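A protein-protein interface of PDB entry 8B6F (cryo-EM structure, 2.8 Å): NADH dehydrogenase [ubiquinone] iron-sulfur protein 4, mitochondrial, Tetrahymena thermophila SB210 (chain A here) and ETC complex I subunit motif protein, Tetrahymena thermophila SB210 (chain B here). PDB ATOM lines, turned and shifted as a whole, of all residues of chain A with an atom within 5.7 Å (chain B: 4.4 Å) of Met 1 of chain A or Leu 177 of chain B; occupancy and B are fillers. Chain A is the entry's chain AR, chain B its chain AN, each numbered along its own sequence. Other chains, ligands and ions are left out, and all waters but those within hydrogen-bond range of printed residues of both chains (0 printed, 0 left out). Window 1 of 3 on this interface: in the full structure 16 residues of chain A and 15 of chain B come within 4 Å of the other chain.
O of Val 175 of chain B lies within hydrogen-bond range of N of Leu 2 of chain A (2.7 Å). The side-chain hydroxyl (OH) of Tyr 103 of chain A sits at hydrogen-bond distance from a ring nitrogen (NE2) of His 179 of chain B (2.9 Å). The backbone carbonyl oxygen (O) of Val 175 of chain B lies within hydrogen-bond range of the backbone NH (N) of Met 1 of chain A (3.2 Å).
The backbone NH of Lys 104 of chain A is in hydrogen-bond range of the side-chain sulfur of Met 1 of chain A.
Among the printed residues, pairs that only touch across the chains: Met 1 of chain A with Tyr 176 of chain B, Met 1 of chain A with Leu 177 of chain B, Leu 2 of chain A with Leu 177 of chain B, Leu 2 of chain A with Gln 180 of chain B, Ile 87 of chain A with Leu 177 of chain B, Tyr 103 of chain A with Tyr 176 of chain B, Tyr 103 of chain A with Lys 178 of chain B and Trp 105 of chain A with Leu 177 of chain B.
Met 1 of chain A touches just these residues of chain B: Val 175 (3.2 Å), Tyr 176 (3.6 Å) and Leu 177 (3.3 Å). Of the printed residues of chain A, Leu 177 of chain B touches Met 1 (3.3 Å), Leu 2 (3.4 Å), Ile 87 (3.8 Å) and Trp 105 (3.9 Å). Of the printed residues of chain A, Tyr 176 of chain B touches Met 1 (3.6 Å) and Tyr 103 (3.5 Å). Of the printed residues of chain A, Val 175 of chain B touches Met 1 and Leu 2. Printed residues of chain B within 4 Å of Leu 2 of chain A: Val 175 (2.7 Å), Leu 177 (3.4 Å) and Gln 180 (3.3 Å). Of the printed residues of chain B, Tyr 103 of chain A touches Tyr 176, Lys 178 and His 179. Printed residues of chain B within 4 Å of Ile 87 of chain A: Leu 177. Pro 158 of chain A touches none of the printed residues of chain B. Leu 3 of chain A touches none of the printed residues of chain B. The nearest residue of chain A that does not touch Leu 177 of chain B is Ala 49 of chain A (4.3 Å).
Of the 14 printed residues of chain A, 5 touch a printed residue of chain B. Of the 6 printed residues of chain B, 6 touch a printed residue of chain A. Printed residues of chain B that touch a printed residue of chain A: Val 175, Tyr 176, Leu 177, Lys 178, His 179 and Gln 180. Hydrophobic or aromatic side chains of chain B that line the printed part of chain A: Val 175, Tyr 176, Leu 177 and His 179.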
ATOM      1  N   MET A   1      -1.120  28.354  26.437  1.00  0.00           N
ATOM      2  CA  MET A   1       0.257  28.552  25.906  1.00  0.00           C
ATOM      3  C   MET A   1       0.281  29.670  24.866  1.00  0.00           C
ATOM      4  O   MET A   1       1.338  30.023  24.349  1.00  0.00           O
ATOM      5  CB  MET A   1       0.786  27.249  25.302  1.00  0.00           C
ATOM      6  CG  MET A   1       2.245  27.307  24.886  1.00  0.00           C
ATOM      7  SD  MET A   1       2.962  25.673  24.651  1.00  0.00           S
ATOM      8  CE  MET A   1       1.959  25.047  23.310  1.00  0.00           C
ATOM      9  N   LEU A   2      -0.894  30.221  24.558  1.00  0.00           N
ATOM     10  CA  LEU A   2      -0.994  31.352  23.636  1.00  0.00           C
ATOM     11  C   LEU A   2      -2.163  32.221  24.085  1.00  0.00           C
ATOM     12  O   LEU A   2      -3.324  31.877  23.840  1.00  0.00           O
ATOM     13  CB  LEU A   2      -1.182  30.891  22.201  1.00  0.00           C
ATOM     14  CG  LEU A   2       0.010  30.259  21.497  1.00  0.00           C
ATOM     15  CD1 LEU A   2      -0.457  29.856  20.124  1.00  0.00           C
ATOM     16  CD2 LEU A   2       1.202  31.202  21.418  1.00  0.00           C
ATOM     17  N   LEU A   3      -1.853  33.335  24.733  1.00  0.00           N
ATOM     18  CA  LEU A   3      -2.879  34.295  25.083  1.00  0.00           C
ATOM     19  C   LEU A   3      -3.314  35.064  23.838  1.00  0.00           C
ATOM     20  O   LEU A   3      -2.608  35.078  22.828  1.00  0.00           O
ATOM     21  CB  LEU A   3      -2.366  35.252  26.152  1.00  0.00           C
ATOM     22  CG  LEU A   3      -2.376  34.706  27.582  1.00  0.00           C
ATOM     23  CD1 LEU A   3      -1.468  33.493  27.733  1.00  0.00           C
ATOM     24  CD2 LEU A   3      -1.980  35.794  28.555  1.00  0.00           C
ATOM     25  N   ALA A  49       6.418  33.819  20.402  1.00  0.00           N
ATOM     26  CA  ALA A  49       6.125  32.444  20.022  1.00  0.00           C
ATOM     27  C   ALA A  49       5.902  32.301  18.524  1.00  0.00           C
ATOM     28  O   ALA A  49       6.012  31.190  17.995  1.00  0.00           O
ATOM     29  CB  ALA A  49       4.898  31.942  20.783  1.00  0.00           C
ATOM     30  N   GLN A  50       5.596  33.394  17.828  1.00  0.00           N
ATOM     31  CA  GLN A  50       5.417  33.367  16.383  1.00  0.00           C
ATOM     32  C   GLN A  50       6.733  33.465  15.626  1.00  0.00           C
ATOM     33  O   GLN A  50       6.726  33.380  14.393  1.00  0.00           O
ATOM     34  CB  GLN A  50       4.487  34.503  15.943  1.00  0.00           C
ATOM     35  CG  GLN A  50       3.022  34.287  16.302  1.00  0.00           C
ATOM     36  CD  GLN A  50       2.762  34.348  17.796  1.00  0.00           C
ATOM     37  OE1 GLN A  50       3.594  34.826  18.564  1.00  0.00           O
ATOM     38  NE2 GLN A  50       1.601  33.857  18.213  1.00  0.00           N
ATOM     39  N   ILE A  87      10.063  23.440  22.662  1.00  0.00           N
ATOM     40  CA  ILE A  87       8.878  22.648  22.968  1.00  0.00           C
ATOM     41  C   ILE A  87       9.205  21.180  22.733  1.00  0.00           C
ATOM     42  O   ILE A  87       9.607  20.793  21.631  1.00  0.00           O
ATOM     43  CB  ILE A  87       7.669  23.093  22.128  1.00  0.00           C
ATOM     44  CG1 ILE A  87       7.152  24.441  22.641  1.00  0.00           C
ATOM     45  CG2 ILE A  87       6.566  22.033  22.151  1.00  0.00           C
ATOM     46  CD1 ILE A  87       5.969  24.986  21.884  1.00  0.00           C
ATOM     47  N   GLY A 102       4.045  18.658  24.684  1.00  0.00           N
ATOM     48  CA  GLY A 102       3.980  19.718  23.702  1.00  0.00           C
ATOM     49  C   GLY A 102       3.107  20.892  24.079  1.00  0.00           C
ATOM     50  O   GLY A 102       2.897  21.777  23.242  1.00  0.00           O
ATOM     51  N   TYR A 103       2.590  20.931  25.305  1.00  0.00           N
ATOM     52  CA  TYR A 103       1.742  22.018  25.774  1.00  0.00           C
ATOM     53  C   TYR A 103       2.496  23.007  26.650  1.00  0.00           C
ATOM     54  O   TYR A 103       1.870  23.869  27.275  1.00  0.00           O
ATOM     55  CB  TYR A 103       0.548  21.456  26.548  1.00  0.00           C
ATOM     56  CG  TYR A 103      -0.356  20.558  25.735  1.00  0.00           C
ATOM     57  CD1 TYR A 103       0.029  19.265  25.412  1.00  0.00           C
ATOM     58  CD2 TYR A 103      -1.601  20.997  25.307  1.00  0.00           C
ATOM     59  CE1 TYR A 103      -0.790  18.440  24.678  1.00  0.00           C
ATOM     60  CE2 TYR A 103      -2.431  20.175  24.570  1.00  0.00           C
ATOM     61  CZ  TYR A 103      -2.018  18.896  24.262  1.00  0.00           C
ATOM     62  OH  TYR A 103      -2.831  18.065  23.531  1.00  0.00           O
ATOM     63  N   LYS A 104       3.820  22.904  26.715  1.00  0.00           N
ATOM     64  CA  LYS A 104       4.607  23.747  27.600  1.00  0.00           C
ATOM     65  C   LYS A 104       6.022  23.849  27.056  1.00  0.00           C
ATOM     66  O   LYS A 104       6.525  22.921  26.418  1.00  0.00           O
ATOM     67  CB  LYS A 104       4.621  23.192  29.028  1.00  0.00           C
ATOM     68  CG  LYS A 104       5.091  21.748  29.127  1.00  0.00           C
ATOM     69  CD  LYS A 104       4.866  21.182  30.518  1.00  0.00           C
ATOM     70  CE  LYS A 104       5.367  19.752  30.623  1.00  0.00           C
ATOM     71  NZ  LYS A 104       4.598  18.826  29.750  1.00  0.00           N
ATOM     72  N   TRP A 105       6.657  24.989  27.320  1.00  0.00           N
ATOM     73  CA  TRP A 105       8.035  25.211  26.908  1.00  0.00           C
ATOM     74  C   TRP A 105       8.974  24.599  27.936  1.00  0.00           C
ATOM     75  O   TRP A 105       8.871  24.883  29.133  1.00  0.00           O
ATOM     76  CB  TRP A 105       8.322  26.704  26.755  1.00  0.00           C
ATOM     77  CG  TRP A 105       7.582  27.349  25.633  1.00  0.00           C
ATOM     78  CD1 TRP A 105       6.292  27.789  25.649  1.00  0.00           C
ATOM     79  CD2 TRP A 105       8.087  27.633  24.324  1.00  0.00           C
ATOM     80  NE1 TRP A 105       5.962  28.328  24.431  1.00  0.00           N
ATOM     81  CE2 TRP A 105       7.046  28.242  23.598  1.00  0.00           C
ATOM     82  CE3 TRP A 105       9.319  27.428  23.695  1.00  0.00           C
ATOM     83  CZ2 TRP A 105       7.199  28.653  22.276  1.00  0.00           C
ATOM     84  CZ3 TRP A 105       9.470  27.835  22.381  1.00  0.00           C
ATOM     85  CH2 TRP A 105       8.415  28.440  21.684  1.00  0.00           C
ATOM     86  N   CYS A 137       4.659  27.775  31.089  1.00  0.00           N
ATOM     87  CA  CYS A 137       3.463  27.816  30.256  1.00  0.00           C
ATOM     88  C   CYS A 137       3.694  28.604  28.974  1.00  0.00           C
ATOM     89  O   CYS A 137       3.141  28.254  27.928  1.00  0.00           O
ATOM     90  CB  CYS A 137       2.292  28.409  31.041  1.00  0.00           C
ATOM     91  SG  CYS A 137       2.577  30.069  31.685  1.00  0.00           S
ATOM     92  N   THR A 138       4.501  29.661  29.033  1.00  0.00           N
ATOM     93  CA  THR A 138       4.725  30.547  27.901  1.00  0.00           C
ATOM     94  C   THR A 138       6.211  30.820  27.724  1.00  0.00           C
ATOM     95  O   THR A 138       6.973  30.870  28.692  1.00  0.00           O
ATOM     96  CB  THR A 138       3.982  31.881  28.068  1.00  0.00           C
ATOM     97  OG1 THR A 138       4.283  32.444  29.351  1.00  0.00           O
ATOM     98  CG2 THR A 138       2.482  31.680  27.940  1.00  0.00           C
ATOM     99  N   PRO A 158       9.329  25.720  17.624  1.00  0.00           N
ATOM    100  CA  PRO A 158       8.809  24.397  17.270  1.00  0.00           C
ATOM    101  C   PRO A 158       8.480  24.276  15.792  1.00  0.00           C
ATOM    102  O   PRO A 158       8.294  25.263  15.076  1.00  0.00           O
ATOM    103  CB  PRO A 158       7.537  24.284  18.116  1.00  0.00           C
ATOM    104  CG  PRO A 158       7.079  25.694  18.254  1.00  0.00           C
ATOM    105  CD  PRO A 158       8.326  26.528  18.340  1.00  0.00           C
ATOM    106  N   SER A 160       5.805  21.814  13.308  1.00  0.00           N
ATOM    107  CA  SER A 160       4.624  20.967  13.377  1.00  0.00           C
ATOM    108  C   SER A 160       4.232  20.517  11.976  1.00  0.00           C
ATOM    109  O   SER A 160       4.718  21.036  10.969  1.00  0.00           O
ATOM    110  CB  SER A 160       3.453  21.695  14.052  1.00  0.00           C
ATOM    111  OG  SER A 160       3.160  22.915  13.392  1.00  0.00           O
ATOM    112  N   VAL B 175      -5.013  29.146  24.128  1.00  0.00           N
ATOM    113  CA  VAL B 175      -4.895  28.090  23.133  1.00  0.00           C
ATOM    114  C   VAL B 175      -3.438  27.649  23.076  1.00  0.00           C
ATOM    115  O   VAL B 175      -2.540  28.327  23.581  1.00  0.00           O
ATOM    116  CB  VAL B 175      -5.384  28.539  21.740  1.00  0.00           C
ATOM    117  CG1 VAL B 175      -6.852  28.923  21.797  1.00  0.00           C
ATOM    118  CG2 VAL B 175      -4.546  29.698  21.220  1.00  0.00           C
ATOM    119  N   TYR B 176      -3.213  26.494  22.455  1.00  0.00           N
ATOM    120  CA  TYR B 176      -1.901  25.863  22.415  1.00  0.00           C
ATOM    121  C   TYR B 176      -1.376  25.796  20.988  1.00  0.00           C
ATOM    122  O   TYR B 176      -2.136  25.556  20.046  1.00  0.00           O
ATOM    123  CB  TYR B 176      -1.958  24.456  23.020  1.00  0.00           C
ATOM    124  CG  TYR B 176      -2.357  24.451  24.478  1.00  0.00           C
ATOM    125  CD1 TYR B 176      -3.694  24.455  24.854  1.00  0.00           C
ATOM    126  CD2 TYR B 176      -1.397  24.452  25.478  1.00  0.00           C
ATOM    127  CE1 TYR B 176      -4.062  24.455  26.186  1.00  0.00           C
ATOM    128  CE2 TYR B 176      -1.754  24.453  26.813  1.00  0.00           C
ATOM    129  CZ  TYR B 176      -3.086  24.455  27.159  1.00  0.00           C
ATOM    130  OH  TYR B 176      -3.443  24.456  28.487  1.00  0.00           O
ATOM    131  N   LEU B 177      -0.066  26.017  20.837  1.00  0.00           N
ATOM    132  CA  LEU B 177       0.558  25.956  19.518  1.00  0.00           C
ATOM    133  C   LEU B 177       0.389  24.589  18.876  1.00  0.00           C
ATOM    134  O   LEU B 177       0.313  24.486  17.646  1.00  0.00           O
ATOM    135  CB  LEU B 177       2.047  26.294  19.628  1.00  0.00           C
ATOM    136  CG  LEU B 177       2.425  27.739  19.933  1.00  0.00           C
ATOM    137  CD1 LEU B 177       3.832  27.823  20.473  1.00  0.00           C
ATOM    138  CD2 LEU B 177       2.360  28.531  18.639  1.00  0.00           C
ATOM    139  N   LYS B 178       0.335  23.528  19.682  1.00  0.00           N
ATOM    140  CA  LYS B 178       0.280  22.186  19.119  1.00  0.00           C
ATOM    141  C   LYS B 178      -0.967  21.997  18.266  1.00  0.00           C
ATOM    142  O   LYS B 178      -0.925  21.321  17.233  1.00  0.00           O
ATOM    143  CB  LYS B 178       0.328  21.148  20.240  1.00  0.00           C
ATOM    144  CG  LYS B 178       0.424  19.715  19.750  1.00  0.00           C
ATOM    145  CD  LYS B 178       0.493  18.734  20.911  1.00  0.00           C
ATOM    146  CE  LYS B 178       0.653  17.308  20.411  1.00  0.00           C
ATOM    147  NZ  LYS B 178       0.702  16.326  21.528  1.00  0.00           N
ATOM    148  N   HIS B 179      -2.086  22.587  18.681  1.00  0.00           N
ATOM    149  CA  HIS B 179      -3.356  22.413  17.993  1.00  0.00           C
ATOM    150  C   HIS B 179      -3.644  23.505  16.971  1.00  0.00           C
ATOM    151  O   HIS B 179      -4.718  23.489  16.362  1.00  0.00           O
ATOM    152  CB  HIS B 179      -4.496  22.363  19.010  1.00  0.00           C
ATOM    153  CG  HIS B 179      -4.352  21.265  20.016  1.00  0.00           C
ATOM    154  ND1 HIS B 179      -4.395  19.931  19.673  1.00  0.00           N
ATOM    155  CD2 HIS B 179      -4.170  21.305  21.356  1.00  0.00           C
ATOM    156  CE1 HIS B 179      -4.241  19.195  20.759  1.00  0.00           C
ATOM    157  NE2 HIS B 179      -4.103  20.005  21.794  1.00  0.00           N
ATOM    158  N   GLN B 180      -2.726  24.444  16.765  1.00  0.00           N
ATOM    159  CA  GLN B 180      -2.930  25.489  15.773  1.00  0.00           C
ATOM    160  C   GLN B 180      -2.543  24.979  14.392  1.00  0.00           C
ATOM    161  O   GLN B 180      -1.454  24.428  14.204  1.00  0.00           O
ATOM    162  CB  GLN B 180      -2.120  26.735  16.125  1.00  0.00           C
ATOM    163  CG  GLN B 180      -2.757  27.590  17.206  1.00  0.00           C
ATOM    164  CD  GLN B 180      -2.091  28.945  17.336  1.00  0.00           C
ATOM    165  OE1 GLN B 180      -0.936  29.121  16.949  1.00  0.00           O
ATOM    166  NE2 GLN B 180      -2.821  29.913  17.878  1.00  0.00           N
